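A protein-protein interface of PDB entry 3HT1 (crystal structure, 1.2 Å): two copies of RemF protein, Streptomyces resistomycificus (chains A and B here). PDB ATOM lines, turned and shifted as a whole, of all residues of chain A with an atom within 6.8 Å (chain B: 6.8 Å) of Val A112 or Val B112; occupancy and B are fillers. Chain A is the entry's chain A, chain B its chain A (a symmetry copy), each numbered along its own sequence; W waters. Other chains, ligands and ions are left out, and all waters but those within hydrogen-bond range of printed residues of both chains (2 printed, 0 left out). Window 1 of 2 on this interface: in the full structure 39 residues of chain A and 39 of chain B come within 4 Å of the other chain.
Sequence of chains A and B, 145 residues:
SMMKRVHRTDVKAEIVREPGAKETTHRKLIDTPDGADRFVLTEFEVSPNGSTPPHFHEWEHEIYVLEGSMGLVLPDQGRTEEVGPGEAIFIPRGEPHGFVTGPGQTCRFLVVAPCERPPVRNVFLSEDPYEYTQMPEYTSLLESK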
ATOM      1  N   PHE A  39      -8.404 -21.199  -5.743  1.00  0.00           N
ATOM      2  CA  PHE A  39      -7.274 -21.973  -6.206  1.00  0.00           C
ATOM      3  C   PHE A  39      -7.768 -22.957  -7.262  1.00  0.00           C
ATOM      4  O   PHE A  39      -8.956 -23.298  -7.296  1.00  0.00           O
ATOM      5  CB  PHE A  39      -6.545 -22.686  -5.048  1.00  0.00           C
ATOM      6  CG  PHE A  39      -7.475 -23.440  -4.123  1.00  0.00           C
ATOM      7  CD1 PHE A  39      -7.885 -24.740  -4.402  1.00  0.00           C
ATOM      8  CD2 PHE A  39      -7.952 -22.856  -2.958  1.00  0.00           C
ATOM      9  CE1 PHE A  39      -8.754 -25.403  -3.532  1.00  0.00           C
ATOM     10  CE2 PHE A  39      -8.791 -23.491  -2.108  1.00  0.00           C
ATOM     11  CZ  PHE A  39      -9.194 -24.768  -2.408  1.00  0.00           C
ATOM     12  N   VAL A  40      -6.847 -23.389  -8.097  1.00  0.00           N
ATOM     13  CA  VAL A  40      -7.134 -24.234  -9.253  1.00  0.00           C
ATOM     14  C   VAL A  40      -6.141 -25.393  -9.283  1.00  0.00           C
ATOM     15  O   VAL A  40      -5.103 -25.358  -8.634  1.00  0.00           O
ATOM     16  CB  VAL A  40      -7.077 -23.445 -10.578  1.00  0.00           C
ATOM     17  CG1 VAL A  40      -8.154 -22.344 -10.562  1.00  0.00           C
ATOM     18  CG2 VAL A  40      -5.697 -22.856 -10.834  1.00  0.00           C
ATOM     19  N   LEU A  41      -6.444 -26.437 -10.050  1.00  0.00           N
ATOM     20  CA  LEU A  41      -5.701 -27.671 -10.125  1.00  0.00           C
ATOM     21  C   LEU A  41      -5.407 -28.008 -11.579  1.00  0.00           C
ATOM     22  O   LEU A  41      -6.324 -28.152 -12.366  1.00  0.00           O
ATOM     23  CB  LEU A  41      -6.492 -28.812  -9.460  1.00  0.00           C
ATOM     24  CG  LEU A  41      -5.731 -30.149  -9.404  1.00  0.00           C
ATOM     25  CD1 LEU A  41      -4.579 -30.042  -8.433  1.00  0.00           C
ATOM     26  CD2 LEU A  41      -6.718 -31.250  -9.026  1.00  0.00           C
ATOM     27  N   THR A  42      -4.119 -28.111 -11.916  1.00  0.00           N
ATOM     28  CA  THR A  42      -3.683 -28.350 -13.296  1.00  0.00           C
ATOM     29  C   THR A  42      -2.711 -29.500 -13.310  1.00  0.00           C
ATOM     30  O   THR A  42      -1.826 -29.581 -12.455  1.00  0.00           O
ATOM     31  CB  THR A  42      -3.013 -27.082 -13.868  1.00  0.00           C
ATOM     32  OG1 THR A  42      -3.955 -25.998 -13.721  1.00  0.00           O
ATOM     33  CG2 THR A  42      -2.615 -27.200 -15.308  1.00  0.00           C
ATOM     34  N   TRP A  59       3.498 -15.773  -6.600  1.00  0.00           N
ATOM     35  CA  TRP A  59       2.451 -16.745  -6.302  1.00  0.00           C
ATOM     36  C   TRP A  59       3.173 -18.075  -6.084  1.00  0.00           C
ATOM     37  O   TRP A  59       4.038 -18.433  -6.879  1.00  0.00           O
ATOM     38  CB  TRP A  59       1.406 -16.794  -7.376  1.00  0.00           C
ATOM     39  CG  TRP A  59       1.696 -16.844  -8.837  1.00  0.00           C
ATOM     40  CD1 TRP A  59       2.043 -15.763  -9.617  1.00  0.00           C
ATOM     41  CD2 TRP A  59       1.656 -17.960  -9.731  1.00  0.00           C
ATOM     42  NE1 TRP A  59       2.235 -16.143 -10.930  1.00  0.00           N
ATOM     43  CE2 TRP A  59       1.991 -17.499 -11.032  1.00  0.00           C
ATOM     44  CE3 TRP A  59       1.353 -19.333  -9.564  1.00  0.00           C
ATOM     45  CZ2 TRP A  59       2.037 -18.368 -12.111  1.00  0.00           C
ATOM     46  CZ3 TRP A  59       1.401 -20.186 -10.678  1.00  0.00           C
ATOM     47  CH2 TRP A  59       1.729 -19.682 -11.918  1.00  0.00           C
ATOM     48  N   GLU A  60       2.814 -18.750  -5.029  1.00  0.00           N
ATOM     49  CA  GLU A  60       3.412 -19.984  -4.624  1.00  0.00           C
ATOM     50  C   GLU A  60       2.924 -21.145  -5.499  1.00  0.00           C
ATOM     51  O   GLU A  60       1.825 -21.108  -6.035  1.00  0.00           O
ATOM     52  CB  GLU A  60       3.095 -20.243  -3.159  1.00  0.00           C
ATOM     53  CG  GLU A  60       1.654 -20.391  -2.768  1.00  0.00           C
ATOM     54  CD  GLU A  60       0.885 -19.111  -2.458  1.00  0.00           C
ATOM     55  OE1 GLU A  60       1.290 -18.029  -2.965  1.00  0.00           O
ATOM     56  OE2 GLU A  60      -0.144 -19.194  -1.753  1.00  0.00           O
ATOM     57  N   HIS A  61       3.756 -22.179  -5.592  1.00  0.00           N
ATOM     58  CA  HIS A  61       3.378 -23.458  -6.158  1.00  0.00           C
ATOM     59  C   HIS A  61       3.293 -24.545  -5.112  1.00  0.00           C
ATOM     60  O   HIS A  61       4.141 -24.597  -4.223  1.00  0.00           O
ATOM     61  CB  HIS A  61       4.378 -23.995  -7.200  1.00  0.00           C
ATOM     62  CG  HIS A  61       4.501 -23.299  -8.489  1.00  0.00           C
ATOM     63  ND1 HIS A  61       3.452 -23.000  -9.310  1.00  0.00           N
ATOM     64  CD2 HIS A  61       5.599 -22.860  -9.193  1.00  0.00           C
ATOM     65  CE1 HIS A  61       3.905 -22.429 -10.415  1.00  0.00           C
ATOM     66  NE2 HIS A  61       5.200 -22.321 -10.405  1.00  0.00           N
ATOM     67  N   GLU A  62       2.275 -25.375  -5.209  1.00  0.00           N
ATOM     68  CA  GLU A  62       2.215 -26.643  -4.477  1.00  0.00           C
ATOM     69  C   GLU A  62       2.101 -27.725  -5.559  1.00  0.00           C
ATOM     70  O   GLU A  62       1.182 -27.682  -6.390  1.00  0.00           O
ATOM     71  CB  GLU A  62       1.076 -26.709  -3.485  1.00  0.00           C
ATOM     72  CG  GLU A  62       1.244 -25.733  -2.371  1.00  0.00           C
ATOM     73  CD  GLU A  62       0.152 -25.665  -1.335  1.00  0.00           C
ATOM     74  OE1 GLU A  62      -0.738 -26.507  -1.316  1.00  0.00           O
ATOM     75  OE2 GLU A  62       0.227 -24.645  -0.577  1.00  0.00           O
ATOM     76  N   ILE A  63       3.046 -28.649  -5.559  1.00  0.00           N
ATOM     77  CA  ILE A  63       3.222 -29.647  -6.614  1.00  0.00           C
ATOM     78  C   ILE A  63       3.165 -31.028  -6.035  1.00  0.00           C
ATOM     79  O   ILE A  63       3.697 -31.269  -4.942  1.00  0.00           O
ATOM     80  CB  ILE A  63       4.563 -29.401  -7.330  1.00  0.00           C
ATOM     81  CG1 ILE A  63       4.527 -28.046  -8.073  1.00  0.00           C
ATOM     82  CG2 ILE A  63       4.964 -30.519  -8.240  1.00  0.00           C
ATOM     83  CD1 ILE A  63       5.890 -27.531  -8.461  1.00  0.00           C
ATOM     84  N   TYR A  64       2.562 -31.960  -6.755  1.00  0.00           N
ATOM     85  CA  TYR A  64       2.636 -33.384  -6.408  1.00  0.00           C
ATOM     86  C   TYR A  64       3.018 -34.151  -7.651  1.00  0.00           C
ATOM     87  O   TYR A  64       2.324 -34.067  -8.667  1.00  0.00           O
ATOM     88  CB  TYR A  64       1.285 -33.866  -5.861  1.00  0.00           C
ATOM     89  CG  TYR A  64       1.337 -35.262  -5.288  1.00  0.00           C
ATOM     90  CD1 TYR A  64       1.528 -35.463  -3.921  1.00  0.00           C
ATOM     91  CD2 TYR A  64       1.160 -36.367  -6.078  1.00  0.00           C
ATOM     92  CE1 TYR A  64       1.565 -36.734  -3.446  1.00  0.00           C
ATOM     93  CE2 TYR A  64       1.168 -37.633  -5.592  1.00  0.00           C
ATOM     94  CZ  TYR A  64       1.377 -37.832  -4.254  1.00  0.00           C
ATOM     95  OH  TYR A  64       1.382 -39.103  -3.705  1.00  0.00           O
ATOM     96  N   LEU A 110       0.948 -32.632 -10.726  1.00  0.00           N
ATOM     97  CA  LEU A 110      -0.060 -31.644 -10.399  1.00  0.00           C
ATOM     98  C   LEU A 110       0.536 -30.377  -9.868  1.00  0.00           C
ATOM     99  O   LEU A 110       1.486 -30.409  -9.088  1.00  0.00           O
ATOM    100  CB  LEU A 110      -1.013 -32.203  -9.319  1.00  0.00           C
ATOM    101  CG  LEU A 110      -1.791 -33.438  -9.727  1.00  0.00           C
ATOM    102  CD1 LEU A 110      -2.533 -34.037  -8.517  1.00  0.00           C
ATOM    103  CD2 LEU A 110      -2.803 -33.127 -10.830  1.00  0.00           C
ATOM    104  N   VAL A 111      -0.048 -29.256 -10.258  1.00  0.00           N
ATOM    105  CA  VAL A 111       0.236 -27.951  -9.704  1.00  0.00           C
ATOM    106  C   VAL A 111      -1.056 -27.343  -9.181  1.00  0.00           C
ATOM    107  O   VAL A 111      -2.039 -27.234  -9.928  1.00  0.00           O
ATOM    108  CB  VAL A 111       0.866 -27.010 -10.723  1.00  0.00           C
ATOM    109  CG1 VAL A 111       1.068 -25.615 -10.128  1.00  0.00           C
ATOM    110  CG2 VAL A 111       2.177 -27.568 -11.267  1.00  0.00           C
ATOM    111  N   VAL A 112      -1.062 -26.942  -7.948  1.00  0.00           N
ATOM    112  CA  VAL A 112      -2.121 -26.120  -7.351  1.00  0.00           C
ATOM    113  C   VAL A 112      -1.665 -24.678  -7.419  1.00  0.00           C
ATOM    114  O   VAL A 112      -0.529 -24.382  -7.030  1.00  0.00           O
ATOM    115  CB  VAL A 112      -2.382 -26.494  -5.904  1.00  0.00           C
ATOM    116  CG1 VAL A 112      -3.617 -25.726  -5.406  1.00  0.00           C
ATOM    117  CG2 VAL A 112      -2.554 -27.997  -5.754  1.00  0.00           C
ATOM    118  N   ALA A 113      -2.543 -23.789  -7.892  1.00  0.00           N
ATOM    119  CA  ALA A 113      -2.215 -22.392  -8.051  1.00  0.00           C
ATOM    120  C   ALA A 113      -3.347 -21.525  -7.525  1.00  0.00           C
ATOM    121  O   ALA A 113      -4.489 -21.934  -7.603  1.00  0.00           O
ATOM    122  CB  ALA A 113      -1.971 -22.036  -9.510  1.00  0.00           C
ATOM    123  N   PRO A 114      -3.050 -20.307  -7.108  1.00  0.00           N
ATOM    124  CA  PRO A 114      -4.079 -19.328  -6.817  1.00  0.00           C
ATOM    125  C   PRO A 114      -4.754 -18.924  -8.113  1.00  0.00           C
ATOM    126  O   PRO A 114      -4.174 -19.029  -9.183  1.00  0.00           O
ATOM    127  CB  PRO A 114      -3.324 -18.117  -6.274  1.00  0.00           C
ATOM    128  CG  PRO A 114      -2.026 -18.197  -7.006  1.00  0.00           C
ATOM    129  CD  PRO A 114      -1.701 -19.682  -7.004  1.00  0.00           C
ATOM    130  N   PHE B  39      -3.546 -21.934   0.606  1.00  0.00           N
ATOM    131  CA  PHE B  39      -4.110 -23.248   0.395  1.00  0.00           C
ATOM    132  C   PHE B  39      -3.067 -24.287   0.796  1.00  0.00           C
ATOM    133  O   PHE B  39      -1.865 -23.996   0.814  1.00  0.00           O
ATOM    134  CB  PHE B  39      -4.592 -23.446  -1.058  1.00  0.00           C
ATOM    135  CG  PHE B  39      -3.568 -23.036  -2.095  1.00  0.00           C
ATOM    136  CD1 PHE B  39      -2.569 -23.907  -2.517  1.00  0.00           C
ATOM    137  CD2 PHE B  39      -3.593 -21.770  -2.661  1.00  0.00           C
ATOM    138  CE1 PHE B  39      -1.633 -23.492  -3.467  1.00  0.00           C
ATOM    139  CE2 PHE B  39      -2.693 -21.359  -3.584  1.00  0.00           C
ATOM    140  CZ  PHE B  39      -1.708 -22.229  -3.978  1.00  0.00           C
ATOM    141  N   VAL B  40      -3.549 -25.471   1.109  1.00  0.00           N
ATOM    142  CA  VAL B  40      -2.737 -26.563   1.639  1.00  0.00           C
ATOM    143  C   VAL B  40      -3.067 -27.845   0.880  1.00  0.00           C
ATOM    144  O   VAL B  40      -4.089 -27.943   0.210  1.00  0.00           O
ATOM    145  CB  VAL B  40      -2.953 -26.766   3.153  1.00  0.00           C
ATOM    146  CG1 VAL B  40      -2.520 -25.493   3.904  1.00  0.00           C
ATOM    147  CG2 VAL B  40      -4.394 -27.130   3.482  1.00  0.00           C
ATOM    148  N   LEU B  41      -2.207 -28.854   0.982  1.00  0.00           N
ATOM    149  CA  LEU B  41      -2.278 -30.098   0.256  1.00  0.00           C
ATOM    150  C   LEU B  41      -2.163 -31.267   1.223  1.00  0.00           C
ATOM    151  O   LEU B  41      -1.177 -31.377   1.929  1.00  0.00           O
ATOM    152  CB  LEU B  41      -1.159 -30.166  -0.800  1.00  0.00           C
ATOM    153  CG  LEU B  41      -1.218 -31.418  -1.692  1.00  0.00           C
ATOM    154  CD1 LEU B  41      -2.420 -31.341  -2.604  1.00  0.00           C
ATOM    155  CD2 LEU B  41       0.096 -31.524  -2.461  1.00  0.00           C
ATOM    156  N   THR B  42      -3.193 -32.118   1.252  1.00  0.00           N
ATOM    157  CA  THR B  42      -3.259 -33.243   2.191  1.00  0.00           C
ATOM    158  C   THR B  42      -3.578 -34.499   1.427  1.00  0.00           C
ATOM    159  O   THR B  42      -4.442 -34.495   0.547  1.00  0.00           O
ATOM    160  CB  THR B  42      -4.344 -32.981   3.258  1.00  0.00           C
ATOM    161  OG1 THR B  42      -4.041 -31.710   3.872  1.00  0.00           O
ATOM    162  CG2 THR B  42      -4.423 -34.037   4.318  1.00  0.00           C
ATOM    163  N   TRP B  59     -16.332 -24.101   2.517  1.00  0.00           N
ATOM    164  CA  TRP B  59     -15.013 -24.133   1.894  1.00  0.00           C
ATOM    165  C   TRP B  59     -15.065 -25.274   0.877  1.00  0.00           C
ATOM    166  O   TRP B  59     -15.539 -26.359   1.206  1.00  0.00           O
ATOM    167  CB  TRP B  59     -13.916 -24.275   2.906  1.00  0.00           C
ATOM    168  CG  TRP B  59     -13.929 -25.246   4.038  1.00  0.00           C
ATOM    169  CD1 TRP B  59     -14.614 -25.080   5.221  1.00  0.00           C
ATOM    170  CD2 TRP B  59     -13.248 -26.497   4.167  1.00  0.00           C
ATOM    171  NE1 TRP B  59     -14.412 -26.154   6.064  1.00  0.00           N
ATOM    172  CE2 TRP B  59     -13.558 -27.043   5.439  1.00  0.00           C
ATOM    173  CE3 TRP B  59     -12.374 -27.224   3.321  1.00  0.00           C
ATOM    174  CZ2 TRP B  59     -13.038 -28.263   5.843  1.00  0.00           C
ATOM    175  CZ3 TRP B  59     -11.857 -28.451   3.762  1.00  0.00           C
ATOM    176  CH2 TRP B  59     -12.192 -28.931   5.010  1.00  0.00           C
ATOM    177  N   GLU B  60     -14.596 -25.000  -0.307  1.00  0.00           N
ATOM    178  CA  GLU B  60     -14.612 -25.915  -1.407  1.00  0.00           C
ATOM    179  C   GLU B  60     -13.520 -26.980  -1.252  1.00  0.00           C
ATOM    180  O   GLU B  60     -12.495 -26.742  -0.627  1.00  0.00           O
ATOM    181  CB  GLU B  60     -14.433 -25.145  -2.707  1.00  0.00           C
ATOM    182  CG  GLU B  60     -13.163 -24.370  -2.894  1.00  0.00           C
ATOM    183  CD  GLU B  60     -13.125 -22.952  -2.332  1.00  0.00           C
ATOM    184  OE1 GLU B  60     -13.903 -22.663  -1.382  1.00  0.00           O
ATOM    185  OE2 GLU B  60     -12.291 -22.150  -2.805  1.00  0.00           O
ATOM    186  N   HIS B  61     -13.758 -28.135  -1.867  1.00  0.00           N
ATOM    187  CA  HIS B  61     -12.754 -29.164  -2.047  1.00  0.00           C
ATOM    188  C   HIS B  61     -12.334 -29.309  -3.491  1.00  0.00           C
ATOM    189  O   HIS B  61     -13.185 -29.248  -4.377  1.00  0.00           O
ATOM    190  CB  HIS B  61     -13.226 -30.571  -1.633  1.00  0.00           C
ATOM    191  CG  HIS B  61     -13.462 -30.849  -0.209  1.00  0.00           C
ATOM    192  ND1 HIS B  61     -12.560 -30.609   0.787  1.00  0.00           N
ATOM    193  CD2 HIS B  61     -14.520 -31.435   0.447  1.00  0.00           C
ATOM    194  CE1 HIS B  61     -13.055 -31.025   1.941  1.00  0.00           C
ATOM    195  NE2 HIS B  61     -14.240 -31.540   1.799  1.00  0.00           N
ATOM    196  N   GLU B  62     -11.047 -29.472  -3.714  1.00  0.00           N
ATOM    197  CA  GLU B  62     -10.519 -29.927  -5.004  1.00  0.00           C
ATOM    198  C   GLU B  62      -9.760 -31.223  -4.691  1.00  0.00           C
ATOM    199  O   GLU B  62      -8.852 -31.226  -3.846  1.00  0.00           O
ATOM    200  CB  GLU B  62      -9.640 -28.904  -5.686  1.00  0.00           C
ATOM    201  CG  GLU B  62     -10.402 -27.689  -6.092  1.00  0.00           C
ATOM    202  CD  GLU B  62      -9.632 -26.570  -6.745  1.00  0.00           C
ATOM    203  OE1 GLU B  62      -8.469 -26.737  -7.090  1.00  0.00           O
ATOM    204  OE2 GLU B  62     -10.281 -25.478  -6.819  1.00  0.00           O
ATOM    205  N   ILE B  63     -10.162 -32.304  -5.339  1.00  0.00           N
ATOM    206  CA  ILE B  63      -9.699 -33.659  -5.045  1.00  0.00           C
ATOM    207  C   ILE B  63      -9.099 -34.279  -6.271  1.00  0.00           C
ATOM    208  O   ILE B  63      -9.617 -34.092  -7.381  1.00  0.00           O
ATOM    209  CB  ILE B  63     -10.879 -34.499  -4.521  1.00  0.00           C
ATOM    210  CG1 ILE B  63     -11.361 -33.945  -3.160  1.00  0.00           C
ATOM    211  CG2 ILE B  63     -10.579 -35.962  -4.445  1.00  0.00           C
ATOM    212  CD1 ILE B  63     -12.733 -34.426  -2.761  1.00  0.00           C
ATOM    213  N   TYR B  64      -8.036 -35.047  -6.100  1.00  0.00           N
ATOM    214  CA  TYR B  64      -7.496 -35.883  -7.179  1.00  0.00           C
ATOM    215  C   TYR B  64      -7.292 -37.277  -6.634  1.00  0.00           C
ATOM    216  O   TYR B  64      -6.571 -37.457  -5.649  1.00  0.00           O
ATOM    217  CB  TYR B  64      -6.173 -35.298  -7.692  1.00  0.00           C
ATOM    218  CG  TYR B  64      -5.661 -35.981  -8.937  1.00  0.00           C
ATOM    219  CD1 TYR B  64      -5.939 -35.459 -10.200  1.00  0.00           C
ATOM    220  CD2 TYR B  64      -4.879 -37.103  -8.867  1.00  0.00           C
ATOM    221  CE1 TYR B  64      -5.457 -36.102 -11.294  1.00  0.00           C
ATOM    222  CE2 TYR B  64      -4.376 -37.724  -9.963  1.00  0.00           C
ATOM    223  CZ  TYR B  64      -4.666 -37.224 -11.204  1.00  0.00           C
ATOM    224  OH  TYR B  64      -4.167 -37.812 -12.354  1.00  0.00           O
ATOM    225  N   LEU B 110      -5.722 -36.952  -2.963  1.00  0.00           N
ATOM    226  CA  LEU B 110      -5.344 -35.619  -2.539  1.00  0.00           C
ATOM    227  C   LEU B 110      -6.528 -34.718  -2.370  1.00  0.00           C
ATOM    228  O   LEU B 110      -7.461 -34.749  -3.170  1.00  0.00           O
ATOM    229  CB  LEU B 110      -4.414 -34.977  -3.593  1.00  0.00           C
ATOM    230  CG  LEU B 110      -3.103 -35.704  -3.819  1.00  0.00           C
ATOM    231  CD1 LEU B 110      -2.357 -35.116  -5.032  1.00  0.00           C
ATOM    232  CD2 LEU B 110      -2.196 -35.626  -2.590  1.00  0.00           C
ATOM    233  N   VAL B 111      -6.476 -33.881  -1.346  1.00  0.00           N
ATOM    234  CA  VAL B 111      -7.407 -32.798  -1.128  1.00  0.00           C
ATOM    235  C   VAL B 111      -6.634 -31.491  -1.032  1.00  0.00           C
ATOM    236  O   VAL B 111      -5.713 -31.372  -0.211  1.00  0.00           O
ATOM    237  CB  VAL B 111      -8.240 -32.990   0.133  1.00  0.00           C
ATOM    238  CG1 VAL B 111      -9.148 -31.784   0.379  1.00  0.00           C
ATOM    239  CG2 VAL B 111      -9.049 -34.282   0.079  1.00  0.00           C
ATOM    240  N   VAL B 112      -6.997 -30.532  -1.825  1.00  0.00           N
ATOM    241  CA  VAL B 112      -6.538 -29.143  -1.708  1.00  0.00           C
ATOM    242  C   VAL B 112      -7.591 -28.385  -0.928  1.00  0.00           C
ATOM    243  O   VAL B 112      -8.780 -28.488  -1.254  1.00  0.00           O
ATOM    244  CB  VAL B 112      -6.353 -28.489  -3.064  1.00  0.00           C
ATOM    245  CG1 VAL B 112      -5.700 -27.112  -2.868  1.00  0.00           C
ATOM    246  CG2 VAL B 112      -5.532 -29.376  -3.987  1.00  0.00           C
ATOM    247  N   ALA B 113      -7.162 -27.619   0.080  1.00  0.00           N
ATOM    248  CA  ALA B 113      -8.068 -26.883   0.929  1.00  0.00           C
ATOM    249  C   ALA B 113      -7.555 -25.469   1.141  1.00  0.00           C
ATOM    250  O   ALA B 113      -6.356 -25.270   1.150  1.00  0.00           O
ATOM    251  CB  ALA B 113      -8.229 -27.548   2.288  1.00  0.00           C
ATOM    252  N   PRO B 114      -8.439 -24.527   1.422  1.00  0.00           N
ATOM    253  CA  PRO B 114      -8.033 -23.210   1.873  1.00  0.00           C
ATOM    254  C   PRO B 114      -7.435 -23.329   3.261  1.00  0.00           C
ATOM    255  O   PRO B 114      -7.735 -24.257   3.997  1.00  0.00           O
ATOM    256  CB  PRO B 114      -9.332 -22.415   1.979  1.00  0.00           C
ATOM    257  CG  PRO B 114     -10.322 -23.470   2.344  1.00  0.00           C
ATOM    258  CD  PRO B 114      -9.922 -24.655   1.478  1.00  0.00           C
HETATM  259  O   HOH W   1      -0.623 -21.215  -0.064  1.00  0.00           O
HETATM  260  O   HOH W   2     -11.193 -22.412  -5.233  1.00  0.00           O
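O of Phe A39 lies close to OE2 of Glu B62 (2.6 Å). O of Phe B39 sits close to OE2 of Glu A62 (2.6 Å).
The backbone NH (N) of Val A40 lies within hydrogen-bond range of the backbone carbonyl oxygen (O) of Ala A113 (2.8 Å). O of Glu A62 lies within hydrogen-bond range of N of Val A112 (2.8 Å). The backbone carbonyl oxygen of Tyr A64 is in hydrogen-bond range of the backbone NH of Leu A110, 2.9 Å away. The backbone NH (N) of Val B40 sits at hydrogen-bond distance from the backbone carbonyl oxygen (O) of Ala B113, at 2.8 Å. The backbone carbonyl oxygen (O) of Glu B62 lies within hydrogen-bond range of the backbone NH (N) of Val B112. The backbone carbonyl oxygen (O) of Tyr B64 sits at hydrogen-bond distance from the backbone NH (N) of Leu B110 (2.9 Å).
Phe A39 touches Phe B39. Phe A39 touches Ala B113. N of Pro B114 touches CE2 of Phe A39 (3.7 Å). C of Val A40 touches OE1 of Glu B62, 3.5 Å away. Leu A41 touches Glu B62. Glu A60 touches Phe B39 (OE2 to CE2, 3.8 Å). CG of Tyr A64 touches CD1 of Leu B110 (3.7 Å). CD1 of Leu A110 touches CG of Tyr B64, 3.7 Å away. CD1 of Leu A110 touches CD1 of Leu B110, at 3.7 Å. CE1 of Phe B39 touches CG1 of Val A112 (3.6 Å).
Printed residues of chain B within 4 Å of Val A112: Phe B39 and Val B112. Of the printed residues of chain B, Phe A39 touches Phe B39, Glu B60, Glu B62, Val B112, Ala B113 and Pro B114. Of the printed residues of chain A, Ala B113 touches Phe A39 (3.97 Å). Printed residues of chain A within 4 Å of Leu B41: Glu A62 (3.6 Å). His B61 touches none of the printed residues of chain A. Thr A42 touches none of the printed residues of chain B. The nearest residue of chain B that does not touch Val A112 is Leu B41 (4.6 Å). The nearest residue of chain A that does not touch Val B112 is Leu A41 (4.6 Å). The nearest printed residue of chain B that does not touch Tyr A64 is Leu B41 (4.3 Å).
Hydrophobic or aromatic side chains of chain A within 4 Å of the printed part of chain B: Phe A39, Leu A41, Tyr A64, Leu A110, Val A112 and Pro A114. Along chain A the printed residues that touch a printed residue of chain B span positions 39 to 114. Of the 15 printed residues of chain B, 10 touch a printed residue of chain A. Hydrophobic or aromatic side chains of chain B that line the printed part of chain A: Phe B39, Leu B41, Tyr B64, Leu B110, Val B112 and Pro B114. Among the printed residues, 19 pairs touch across the chains.
Phe B39 touches its own counterpart, Phe A39. Phe A39 touches Glu B62, and with the chains exchanged Glu A62 touches Phe B39. Val A40 touches Glu B62, and with the chains exchanged Glu A62 touches Val B40. Leu B110 touches its own counterpart, Leu A110. 15 positions are printed for both chains.
Water W1 lies within hydrogen-bond range of OE2 of Glu A60 (2.7 Å) and N of Phe B39 (3.1 Å). Water W2 bridges OE2 of Glu B60 (2.7 Å) and N of Phe A39 (3.1 Å).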
